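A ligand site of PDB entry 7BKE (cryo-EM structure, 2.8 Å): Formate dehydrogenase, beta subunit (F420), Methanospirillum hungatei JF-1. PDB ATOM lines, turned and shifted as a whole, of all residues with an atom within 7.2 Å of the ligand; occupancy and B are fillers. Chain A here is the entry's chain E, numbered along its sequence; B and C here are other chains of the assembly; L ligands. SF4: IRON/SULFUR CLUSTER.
The backbone carbonyl oxygen (O) of Ile 333 sits close to a ring nitrogen (ND1) of His 337 (3.4 Å). SG of Cys 311 lies close to OG1 of Thr 313. The backbone carbonyl oxygen of Pro 644 of chain B sits at hydrogen-bond distance from the side-chain hydroxyl of Ser 312, at 2.9 Å. The side-chain sulfur (SG) of Cys 308 sits close to the backbone NH (N) of Gly 645 of chain B (3.7 Å).
An iron atom (FE4) of the ligand is bound by the side-chain sulfur (SG) of Cys 311 (2.1 Å). S2 of the ligand sits close to N of Ser 312, at 3.5 Å. An iron atom (FE2) of the ligand is bound by the side-chain sulfur (SG) of Cys 306, at 2.3 Å. FE1 of the ligand is bound by SG of Cys 308 (2.2 Å). FE3 of the ligand is bound by ND1 of His 337 (2.2 Å).
O of Pro 644 of chain B sits close to S2 of the ligand (3.3 Å). Val 300 touches the ligand. Seven residues have an atom within 4 Å of the ligand: Val 300, Cys 306, Cys 308, Cys 311, Ser 312, His 337 and Pro 644 of chain B. The nearest printed residue that does not touch the ligand is Arg 334 (4.1 Å).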
ATOM      1  N   ARG A 114      33.909 -24.697  23.889  1.00  0.00           N
ATOM      2  CA  ARG A 114      33.286 -23.869  22.868  1.00  0.00           C
ATOM      3  C   ARG A 114      33.637 -22.406  23.007  1.00  0.00           C
ATOM      4  O   ARG A 114      32.953 -21.584  22.403  1.00  0.00           O
ATOM      5  CB  ARG A 114      31.781 -24.029  22.912  1.00  0.00           C
ATOM      6  CG  ARG A 114      31.330 -25.336  22.352  1.00  0.00           C
ATOM      7  CD  ARG A 114      30.038 -25.753  22.966  1.00  0.00           C
ATOM      8  NE  ARG A 114      29.628 -27.051  22.465  1.00  0.00           N
ATOM      9  CZ  ARG A 114      30.128 -28.192  22.900  1.00  0.00           C
ATOM     10  NH1 ARG A 114      31.054 -28.198  23.842  1.00  0.00           N
ATOM     11  NH2 ARG A 114      29.702 -29.326  22.394  1.00  0.00           N
ATOM     12  N   VAL A 300      16.883 -24.683  25.545  1.00  0.00           N
ATOM     13  CA  VAL A 300      18.006 -24.125  24.743  1.00  0.00           C
ATOM     14  C   VAL A 300      18.711 -23.070  25.582  1.00  0.00           C
ATOM     15  O   VAL A 300      19.931 -23.083  25.622  1.00  0.00           O
ATOM     16  CB  VAL A 300      17.562 -23.620  23.353  1.00  0.00           C
ATOM     17  CG1 VAL A 300      18.649 -22.825  22.663  1.00  0.00           C
ATOM     18  CG2 VAL A 300      17.061 -24.748  22.464  1.00  0.00           C
ATOM     19  N   GLU A 301      17.965 -22.201  26.245  1.00  0.00           N
ATOM     20  CA  GLU A 301      18.636 -21.138  26.986  1.00  0.00           C
ATOM     21  C   GLU A 301      19.301 -21.634  28.256  1.00  0.00           C
ATOM     22  O   GLU A 301      20.203 -20.968  28.762  1.00  0.00           O
ATOM     23  CB  GLU A 301      17.655 -20.025  27.342  1.00  0.00           C
ATOM     24  CG  GLU A 301      16.853 -19.490  26.179  1.00  0.00           C
ATOM     25  CD  GLU A 301      17.713 -18.965  25.037  1.00  0.00           C
ATOM     26  OE1 GLU A 301      18.790 -18.398  25.296  1.00  0.00           O
ATOM     27  OE2 GLU A 301      17.287 -19.096  23.869  1.00  0.00           O
ATOM     28  N   CYS A 303      20.613 -24.950  28.544  1.00  0.00           N
ATOM     29  CA  CYS A 303      21.632 -25.946  28.270  1.00  0.00           C
ATOM     30  C   CYS A 303      23.018 -25.307  28.246  1.00  0.00           C
ATOM     31  O   CYS A 303      23.185 -24.259  27.634  1.00  0.00           O
ATOM     32  CB  CYS A 303      21.346 -26.647  26.949  1.00  0.00           C
ATOM     33  SG  CYS A 303      22.380 -28.061  26.619  1.00  0.00           S
ATOM     34  N   ILE A 305      25.489 -26.447  26.593  1.00  0.00           N
ATOM     35  CA  ILE A 305      26.118 -26.776  25.284  1.00  0.00           C
ATOM     36  C   ILE A 305      25.486 -25.945  24.182  1.00  0.00           C
ATOM     37  O   ILE A 305      26.066 -25.826  23.124  1.00  0.00           O
ATOM     38  CB  ILE A 305      26.082 -28.313  25.078  1.00  0.00           C
ATOM     39  CG1 ILE A 305      27.144 -29.003  25.935  1.00  0.00           C
ATOM     40  CG2 ILE A 305      26.192 -28.715  23.618  1.00  0.00           C
ATOM     41  CD1 ILE A 305      26.653 -29.436  27.278  1.00  0.00           C
ATOM     42  N   CYS A 306      24.385 -25.315  24.492  1.00  0.00           N
ATOM     43  CA  CYS A 306      23.686 -24.497  23.486  1.00  0.00           C
ATOM     44  C   CYS A 306      24.231 -23.080  23.600  1.00  0.00           C
ATOM     45  O   CYS A 306      23.756 -22.355  24.439  1.00  0.00           O
ATOM     46  CB  CYS A 306      22.196 -24.609  23.728  1.00  0.00           C
ATOM     47  SG  CYS A 306      21.421 -26.051  22.976  1.00  0.00           S
ATOM     48  N   TYR A 307      25.164 -22.716  22.735  1.00  0.00           N
ATOM     49  CA  TYR A 307      25.859 -21.411  22.806  1.00  0.00           C
ATOM     50  C   TYR A 307      25.629 -20.594  21.560  1.00  0.00           C
ATOM     51  O   TYR A 307      26.320 -19.609  21.420  1.00  0.00           O
ATOM     52  CB  TYR A 307      27.356 -21.642  22.677  1.00  0.00           C
ATOM     53  CG  TYR A 307      27.822 -22.238  21.370  1.00  0.00           C
ATOM     54  CD1 TYR A 307      28.531 -21.473  20.473  1.00  0.00           C
ATOM     55  CD2 TYR A 307      27.562 -23.552  21.046  1.00  0.00           C
ATOM     56  CE1 TYR A 307      28.932 -21.989  19.255  1.00  0.00           C
ATOM     57  CE2 TYR A 307      27.973 -24.092  19.840  1.00  0.00           C
ATOM     58  CZ  TYR A 307      28.661 -23.306  18.949  1.00  0.00           C
ATOM     59  OH  TYR A 307      29.088 -23.817  17.751  1.00  0.00           O
ATOM     60  N   CYS A 308      24.627 -20.904  20.773  1.00  0.00           N
ATOM     61  CA  CYS A 308      24.512 -20.309  19.424  1.00  0.00           C
ATOM     62  C   CYS A 308      23.730 -19.022  19.472  1.00  0.00           C
ATOM     63  O   CYS A 308      22.763 -18.957  20.210  1.00  0.00           O
ATOM     64  CB  CYS A 308      23.832 -21.311  18.503  1.00  0.00           C
ATOM     65  SG  CYS A 308      24.786 -22.828  18.260  1.00  0.00           S
ATOM     66  N   ILE A 309      24.169 -18.032  18.702  1.00  0.00           N
ATOM     67  CA  ILE A 309      23.482 -16.748  18.744  1.00  0.00           C
ATOM     68  C   ILE A 309      22.015 -16.918  18.408  1.00  0.00           C
ATOM     69  O   ILE A 309      21.131 -16.403  19.100  1.00  0.00           O
ATOM     70  CB  ILE A 309      24.159 -15.749  17.791  1.00  0.00           C
ATOM     71  CG1 ILE A 309      25.606 -15.498  18.194  1.00  0.00           C
ATOM     72  CG2 ILE A 309      23.405 -14.460  17.757  1.00  0.00           C
ATOM     73  CD1 ILE A 309      25.765 -15.070  19.603  1.00  0.00           C
ATOM     74  N   GLU A 310      21.727 -17.628  17.324  1.00  0.00           N
ATOM     75  CA  GLU A 310      20.358 -17.982  16.969  1.00  0.00           C
ATOM     76  C   GLU A 310      20.282 -19.482  16.798  1.00  0.00           C
ATOM     77  O   GLU A 310      21.020 -20.064  15.998  1.00  0.00           O
ATOM     78  CB  GLU A 310      19.925 -17.281  15.684  1.00  0.00           C
ATOM     79  CG  GLU A 310      18.500 -17.548  15.311  1.00  0.00           C
ATOM     80  CD  GLU A 310      18.109 -16.861  14.031  1.00  0.00           C
ATOM     81  OE1 GLU A 310      18.970 -16.175  13.445  1.00  0.00           O
ATOM     82  OE2 GLU A 310      16.953 -17.009  13.599  1.00  0.00           O
ATOM     83  N   CYS A 311      19.343 -20.111  17.489  1.00  0.00           N
ATOM     84  CA  CYS A 311      19.191 -21.556  17.373  1.00  0.00           C
ATOM     85  C   CYS A 311      18.646 -21.901  15.998  1.00  0.00           C
ATOM     86  O   CYS A 311      17.888 -21.129  15.475  1.00  0.00           O
ATOM     87  CB  CYS A 311      18.344 -22.074  18.533  1.00  0.00           C
ATOM     88  SG  CYS A 311      18.271 -23.863  18.753  1.00  0.00           S
ATOM     89  N   SER A 312      19.027 -23.039  15.470  1.00  0.00           N
ATOM     90  CA  SER A 312      18.461 -23.523  14.207  1.00  0.00           C
ATOM     91  C   SER A 312      17.006 -23.859  14.442  1.00  0.00           C
ATOM     92  O   SER A 312      16.264 -23.901  13.495  1.00  0.00           O
ATOM     93  CB  SER A 312      19.231 -24.672  13.758  1.00  0.00           C
ATOM     94  OG  SER A 312      20.560 -24.285  13.437  1.00  0.00           O
ATOM     95  N   THR A 313      16.590 -24.077  15.687  1.00  0.00           N
ATOM     96  CA  THR A 313      15.171 -24.279  15.899  1.00  0.00           C
ATOM     97  C   THR A 313      14.365 -23.020  15.633  1.00  0.00           C
ATOM     98  O   THR A 313      13.134 -23.083  15.623  1.00  0.00           O
ATOM     99  CB  THR A 313      14.916 -24.748  17.327  1.00  0.00           C
ATOM    100  OG1 THR A 313      15.552 -23.855  18.245  1.00  0.00           O
ATOM    101  CG2 THR A 313      15.492 -26.129  17.534  1.00  0.00           C
ATOM    102  N   LYS A 314      15.020 -21.880  15.424  1.00  0.00           N
ATOM    103  CA  LYS A 314      14.352 -20.625  15.145  1.00  0.00           C
ATOM    104  C   LYS A 314      14.385 -20.250  13.671  1.00  0.00           C
ATOM    105  O   LYS A 314      13.853 -19.200  13.303  1.00  0.00           O
ATOM    106  CB  LYS A 314      14.995 -19.501  15.956  1.00  0.00           C
ATOM    107  CG  LYS A 314      14.515 -19.421  17.382  1.00  0.00           C
ATOM    108  CD  LYS A 314      15.639 -19.037  18.296  1.00  0.00           C
ATOM    109  CE  LYS A 314      15.111 -18.445  19.584  1.00  0.00           C
ATOM    110  NZ  LYS A 314      16.193 -18.201  20.563  1.00  0.00           N
ATOM    111  N   LYS A 315      14.961 -21.052  12.844  1.00  0.00           N
ATOM    112  CA  LYS A 315      15.118 -20.704  11.438  1.00  0.00           C
ATOM    113  C   LYS A 315      13.923 -21.206  10.638  1.00  0.00           C
ATOM    114  O   LYS A 315      13.567 -22.377  10.763  1.00  0.00           O
ATOM    115  CB  LYS A 315      16.410 -21.284  10.899  1.00  0.00           C
ATOM    116  CG  LYS A 315      17.586 -20.833  11.702  1.00  0.00           C
ATOM    117  CD  LYS A 315      18.894 -21.241  11.099  1.00  0.00           C
ATOM    118  CE  LYS A 315      20.040 -20.609  11.859  1.00  0.00           C
ATOM    119  NZ  LYS A 315      19.646 -19.285  12.372  1.00  0.00           N
ATOM    120  N   PHE A 330      12.135 -30.090  16.058  1.00  0.00           N
ATOM    121  CA  PHE A 330      12.634 -29.258  17.139  1.00  0.00           C
ATOM    122  C   PHE A 330      13.550 -30.042  18.057  1.00  0.00           C
ATOM    123  O   PHE A 330      14.622 -29.557  18.441  1.00  0.00           O
ATOM    124  CB  PHE A 330      11.459 -28.675  17.930  1.00  0.00           C
ATOM    125  CG  PHE A 330      11.855 -27.633  18.939  1.00  0.00           C
ATOM    126  CD1 PHE A 330      11.554 -26.316  18.733  1.00  0.00           C
ATOM    127  CD2 PHE A 330      12.504 -27.980  20.114  1.00  0.00           C
ATOM    128  CE1 PHE A 330      11.907 -25.369  19.655  1.00  0.00           C
ATOM    129  CE2 PHE A 330      12.859 -27.041  21.020  1.00  0.00           C
ATOM    130  CZ  PHE A 330      12.559 -25.742  20.796  1.00  0.00           C
ATOM    131  N   ILE A 333      16.815 -31.571  16.327  1.00  0.00           N
ATOM    132  CA  ILE A 333      17.904 -30.574  16.126  1.00  0.00           C
ATOM    133  C   ILE A 333      18.698 -30.459  17.413  1.00  0.00           C
ATOM    134  O   ILE A 333      19.884 -30.236  17.324  1.00  0.00           O
ATOM    135  CB  ILE A 333      17.341 -29.186  15.748  1.00  0.00           C
ATOM    136  CG1 ILE A 333      16.757 -29.138  14.342  1.00  0.00           C
ATOM    137  CG2 ILE A 333      18.373 -28.090  15.946  1.00  0.00           C
ATOM    138  CD1 ILE A 333      15.951 -27.889  14.075  1.00  0.00           C
ATOM    139  N   ARG A 334      18.093 -30.733  18.558  1.00  0.00           N
ATOM    140  CA  ARG A 334      18.829 -30.727  19.840  1.00  0.00           C
ATOM    141  C   ARG A 334      19.504 -32.069  20.033  1.00  0.00           C
ATOM    142  O   ARG A 334      20.619 -32.059  20.516  1.00  0.00           O
ATOM    143  CB  ARG A 334      17.896 -30.386  20.983  1.00  0.00           C
ATOM    144  CG  ARG A 334      17.159 -29.062  20.855  1.00  0.00           C
ATOM    145  CD  ARG A 334      16.629 -28.716  22.221  1.00  0.00           C
ATOM    146  NE  ARG A 334      17.734 -28.557  23.154  1.00  0.00           N
ATOM    147  CZ  ARG A 334      17.839 -29.173  24.330  1.00  0.00           C
ATOM    148  NH1 ARG A 334      16.881 -29.997  24.733  1.00  0.00           N
ATOM    149  NH2 ARG A 334      18.898 -28.952  25.084  1.00  0.00           N
ATOM    150  N   PHE A 335      18.881 -33.174  19.651  1.00  0.00           N
ATOM    151  CA  PHE A 335      19.571 -34.458  19.733  1.00  0.00           C
ATOM    152  C   PHE A 335      20.814 -34.464  18.870  1.00  0.00           C
ATOM    153  O   PHE A 335      21.853 -35.003  19.260  1.00  0.00           O
ATOM    154  CB  PHE A 335      18.643 -35.593  19.314  1.00  0.00           C
ATOM    155  CG  PHE A 335      17.490 -35.813  20.230  1.00  0.00           C
ATOM    156  CD1 PHE A 335      17.564 -35.457  21.547  1.00  0.00           C
ATOM    157  CD2 PHE A 335      16.325 -36.361  19.762  1.00  0.00           C
ATOM    158  CE1 PHE A 335      16.498 -35.647  22.380  1.00  0.00           C
ATOM    159  CE2 PHE A 335      15.259 -36.560  20.594  1.00  0.00           C
ATOM    160  CZ  PHE A 335      15.350 -36.203  21.900  1.00  0.00           C
ATOM    161  N   ALA A 336      20.730 -33.877  17.685  1.00  0.00           N
ATOM    162  CA  ALA A 336      21.886 -33.854  16.790  1.00  0.00           C
ATOM    163  C   ALA A 336      22.990 -32.973  17.343  1.00  0.00           C
ATOM    164  O   ALA A 336      24.169 -33.302  17.225  1.00  0.00           O
ATOM    165  CB  ALA A 336      21.466 -33.382  15.413  1.00  0.00           C
ATOM    166  N   HIS A 337      22.650 -31.826  17.931  1.00  0.00           N
ATOM    167  CA  HIS A 337      23.685 -30.845  18.329  1.00  0.00           C
ATOM    168  C   HIS A 337      24.236 -31.062  19.725  1.00  0.00           C
ATOM    169  O   HIS A 337      25.379 -30.684  19.936  1.00  0.00           O
ATOM    170  CB  HIS A 337      23.124 -29.440  18.215  1.00  0.00           C
ATOM    171  CG  HIS A 337      22.944 -28.928  16.835  1.00  0.00           C
ATOM    172  ND1 HIS A 337      22.168 -27.825  16.579  1.00  0.00           N
ATOM    173  CD2 HIS A 337      23.425 -29.333  15.655  1.00  0.00           C
ATOM    174  CE1 HIS A 337      22.169 -27.590  15.288  1.00  0.00           C
ATOM    175  NE2 HIS A 337      22.936 -28.493  14.703  1.00  0.00           N
ATOM    176  N   VAL A 338      23.488 -31.645  20.637  1.00  0.00           N
ATOM    177  CA  VAL A 338      23.914 -31.714  22.028  1.00  0.00           C
ATOM    178  C   VAL A 338      24.299 -33.128  22.429  1.00  0.00           C
ATOM    179  O   VAL A 338      25.232 -33.310  23.206  1.00  0.00           O
ATOM    180  CB  VAL A 338      22.810 -31.146  22.952  1.00  0.00           C
ATOM    181  CG1 VAL A 338      23.195 -31.319  24.378  1.00  0.00           C
ATOM    182  CG2 VAL A 338      22.575 -29.696  22.662  1.00  0.00           C
ATOM    183  N   CYS B 643      28.747 -25.830  11.268  1.00  0.00           N
ATOM    184  CA  CYS B 643      28.366 -24.744  12.173  1.00  0.00           C
ATOM    185  C   CYS B 643      26.949 -24.898  12.705  1.00  0.00           C
ATOM    186  O   CYS B 643      25.986 -24.818  11.943  1.00  0.00           O
ATOM    187  CB  CYS B 643      28.498 -23.396  11.472  1.00  0.00           C
ATOM    188  SG  CYS B 643      28.164 -21.996  12.544  1.00  0.00           S
ATOM    189  N   PRO B 644      26.756 -25.121  14.038  1.00  0.00           N
ATOM    190  CA  PRO B 644      25.444 -25.384  14.585  1.00  0.00           C
ATOM    191  C   PRO B 644      24.510 -24.193  14.461  1.00  0.00           C
ATOM    192  O   PRO B 644      23.365 -24.418  14.244  1.00  0.00           O
ATOM    193  CB  PRO B 644      25.710 -25.758  16.031  1.00  0.00           C
ATOM    194  CG  PRO B 644      27.147 -26.118  16.082  1.00  0.00           C
ATOM    195  CD  PRO B 644      27.773 -25.136  15.125  1.00  0.00           C
ATOM    196  N   GLY B 645      25.024 -22.963  14.547  1.00  0.00           N
ATOM    197  CA  GLY B 645      24.187 -21.793  14.524  1.00  0.00           C
ATOM    198  C   GLY B 645      23.809 -21.305  13.157  1.00  0.00           C
ATOM    199  O   GLY B 645      23.050 -20.338  13.049  1.00  0.00           O
ATOM    200  N   GLY B 646      24.306 -21.934  12.097  1.00  0.00           N
ATOM    201  CA  GLY B 646      24.022 -21.484  10.754  1.00  0.00           C
ATOM    202  C   GLY B 646      24.653 -20.150  10.427  1.00  0.00           C
ATOM    203  O   GLY B 646      24.051 -19.344   9.711  1.00  0.00           O
ATOM    204  N   LEU C  50      21.278 -32.033   9.968  1.00  0.00           N
ATOM    205  CA  LEU C  50      19.914 -31.564   9.910  1.00  0.00           C
ATOM    206  C   LEU C  50      19.279 -31.826   8.554  1.00  0.00           C
ATOM    207  O   LEU C  50      18.060 -31.951   8.486  1.00  0.00           O
ATOM    208  CB  LEU C  50      19.851 -30.087  10.263  1.00  0.00           C
ATOM    209  CG  LEU C  50      20.524 -29.698  11.580  1.00  0.00           C
ATOM    210  CD1 LEU C  50      20.084 -28.326  11.997  1.00  0.00           C
ATOM    211  CD2 LEU C  50      20.231 -30.681  12.696  1.00  0.00           C
HETATM  212 FE1  SF4 L   1      22.973 -23.982  18.878  1.00  0.00          FE
HETATM  213 FE2  SF4 L   1      21.862 -25.577  20.788  1.00  0.00          FE
HETATM  214 FE3  SF4 L   1      22.036 -26.464  18.260  1.00  0.00          FE
HETATM  215 FE4  SF4 L   1      20.311 -24.485  18.866  1.00  0.00          FE
HETATM  216  S1  SF4 L   1      20.251 -26.624  19.606  1.00  0.00           S
HETATM  217  S2  SF4 L   1      21.696 -24.539  17.090  1.00  0.00           S
HETATM  218  S3  SF4 L   1      21.465 -23.348  20.434  1.00  0.00           S
HETATM  219  S4  SF4 L   1      23.765 -25.975  19.657  1.00  0.00           S
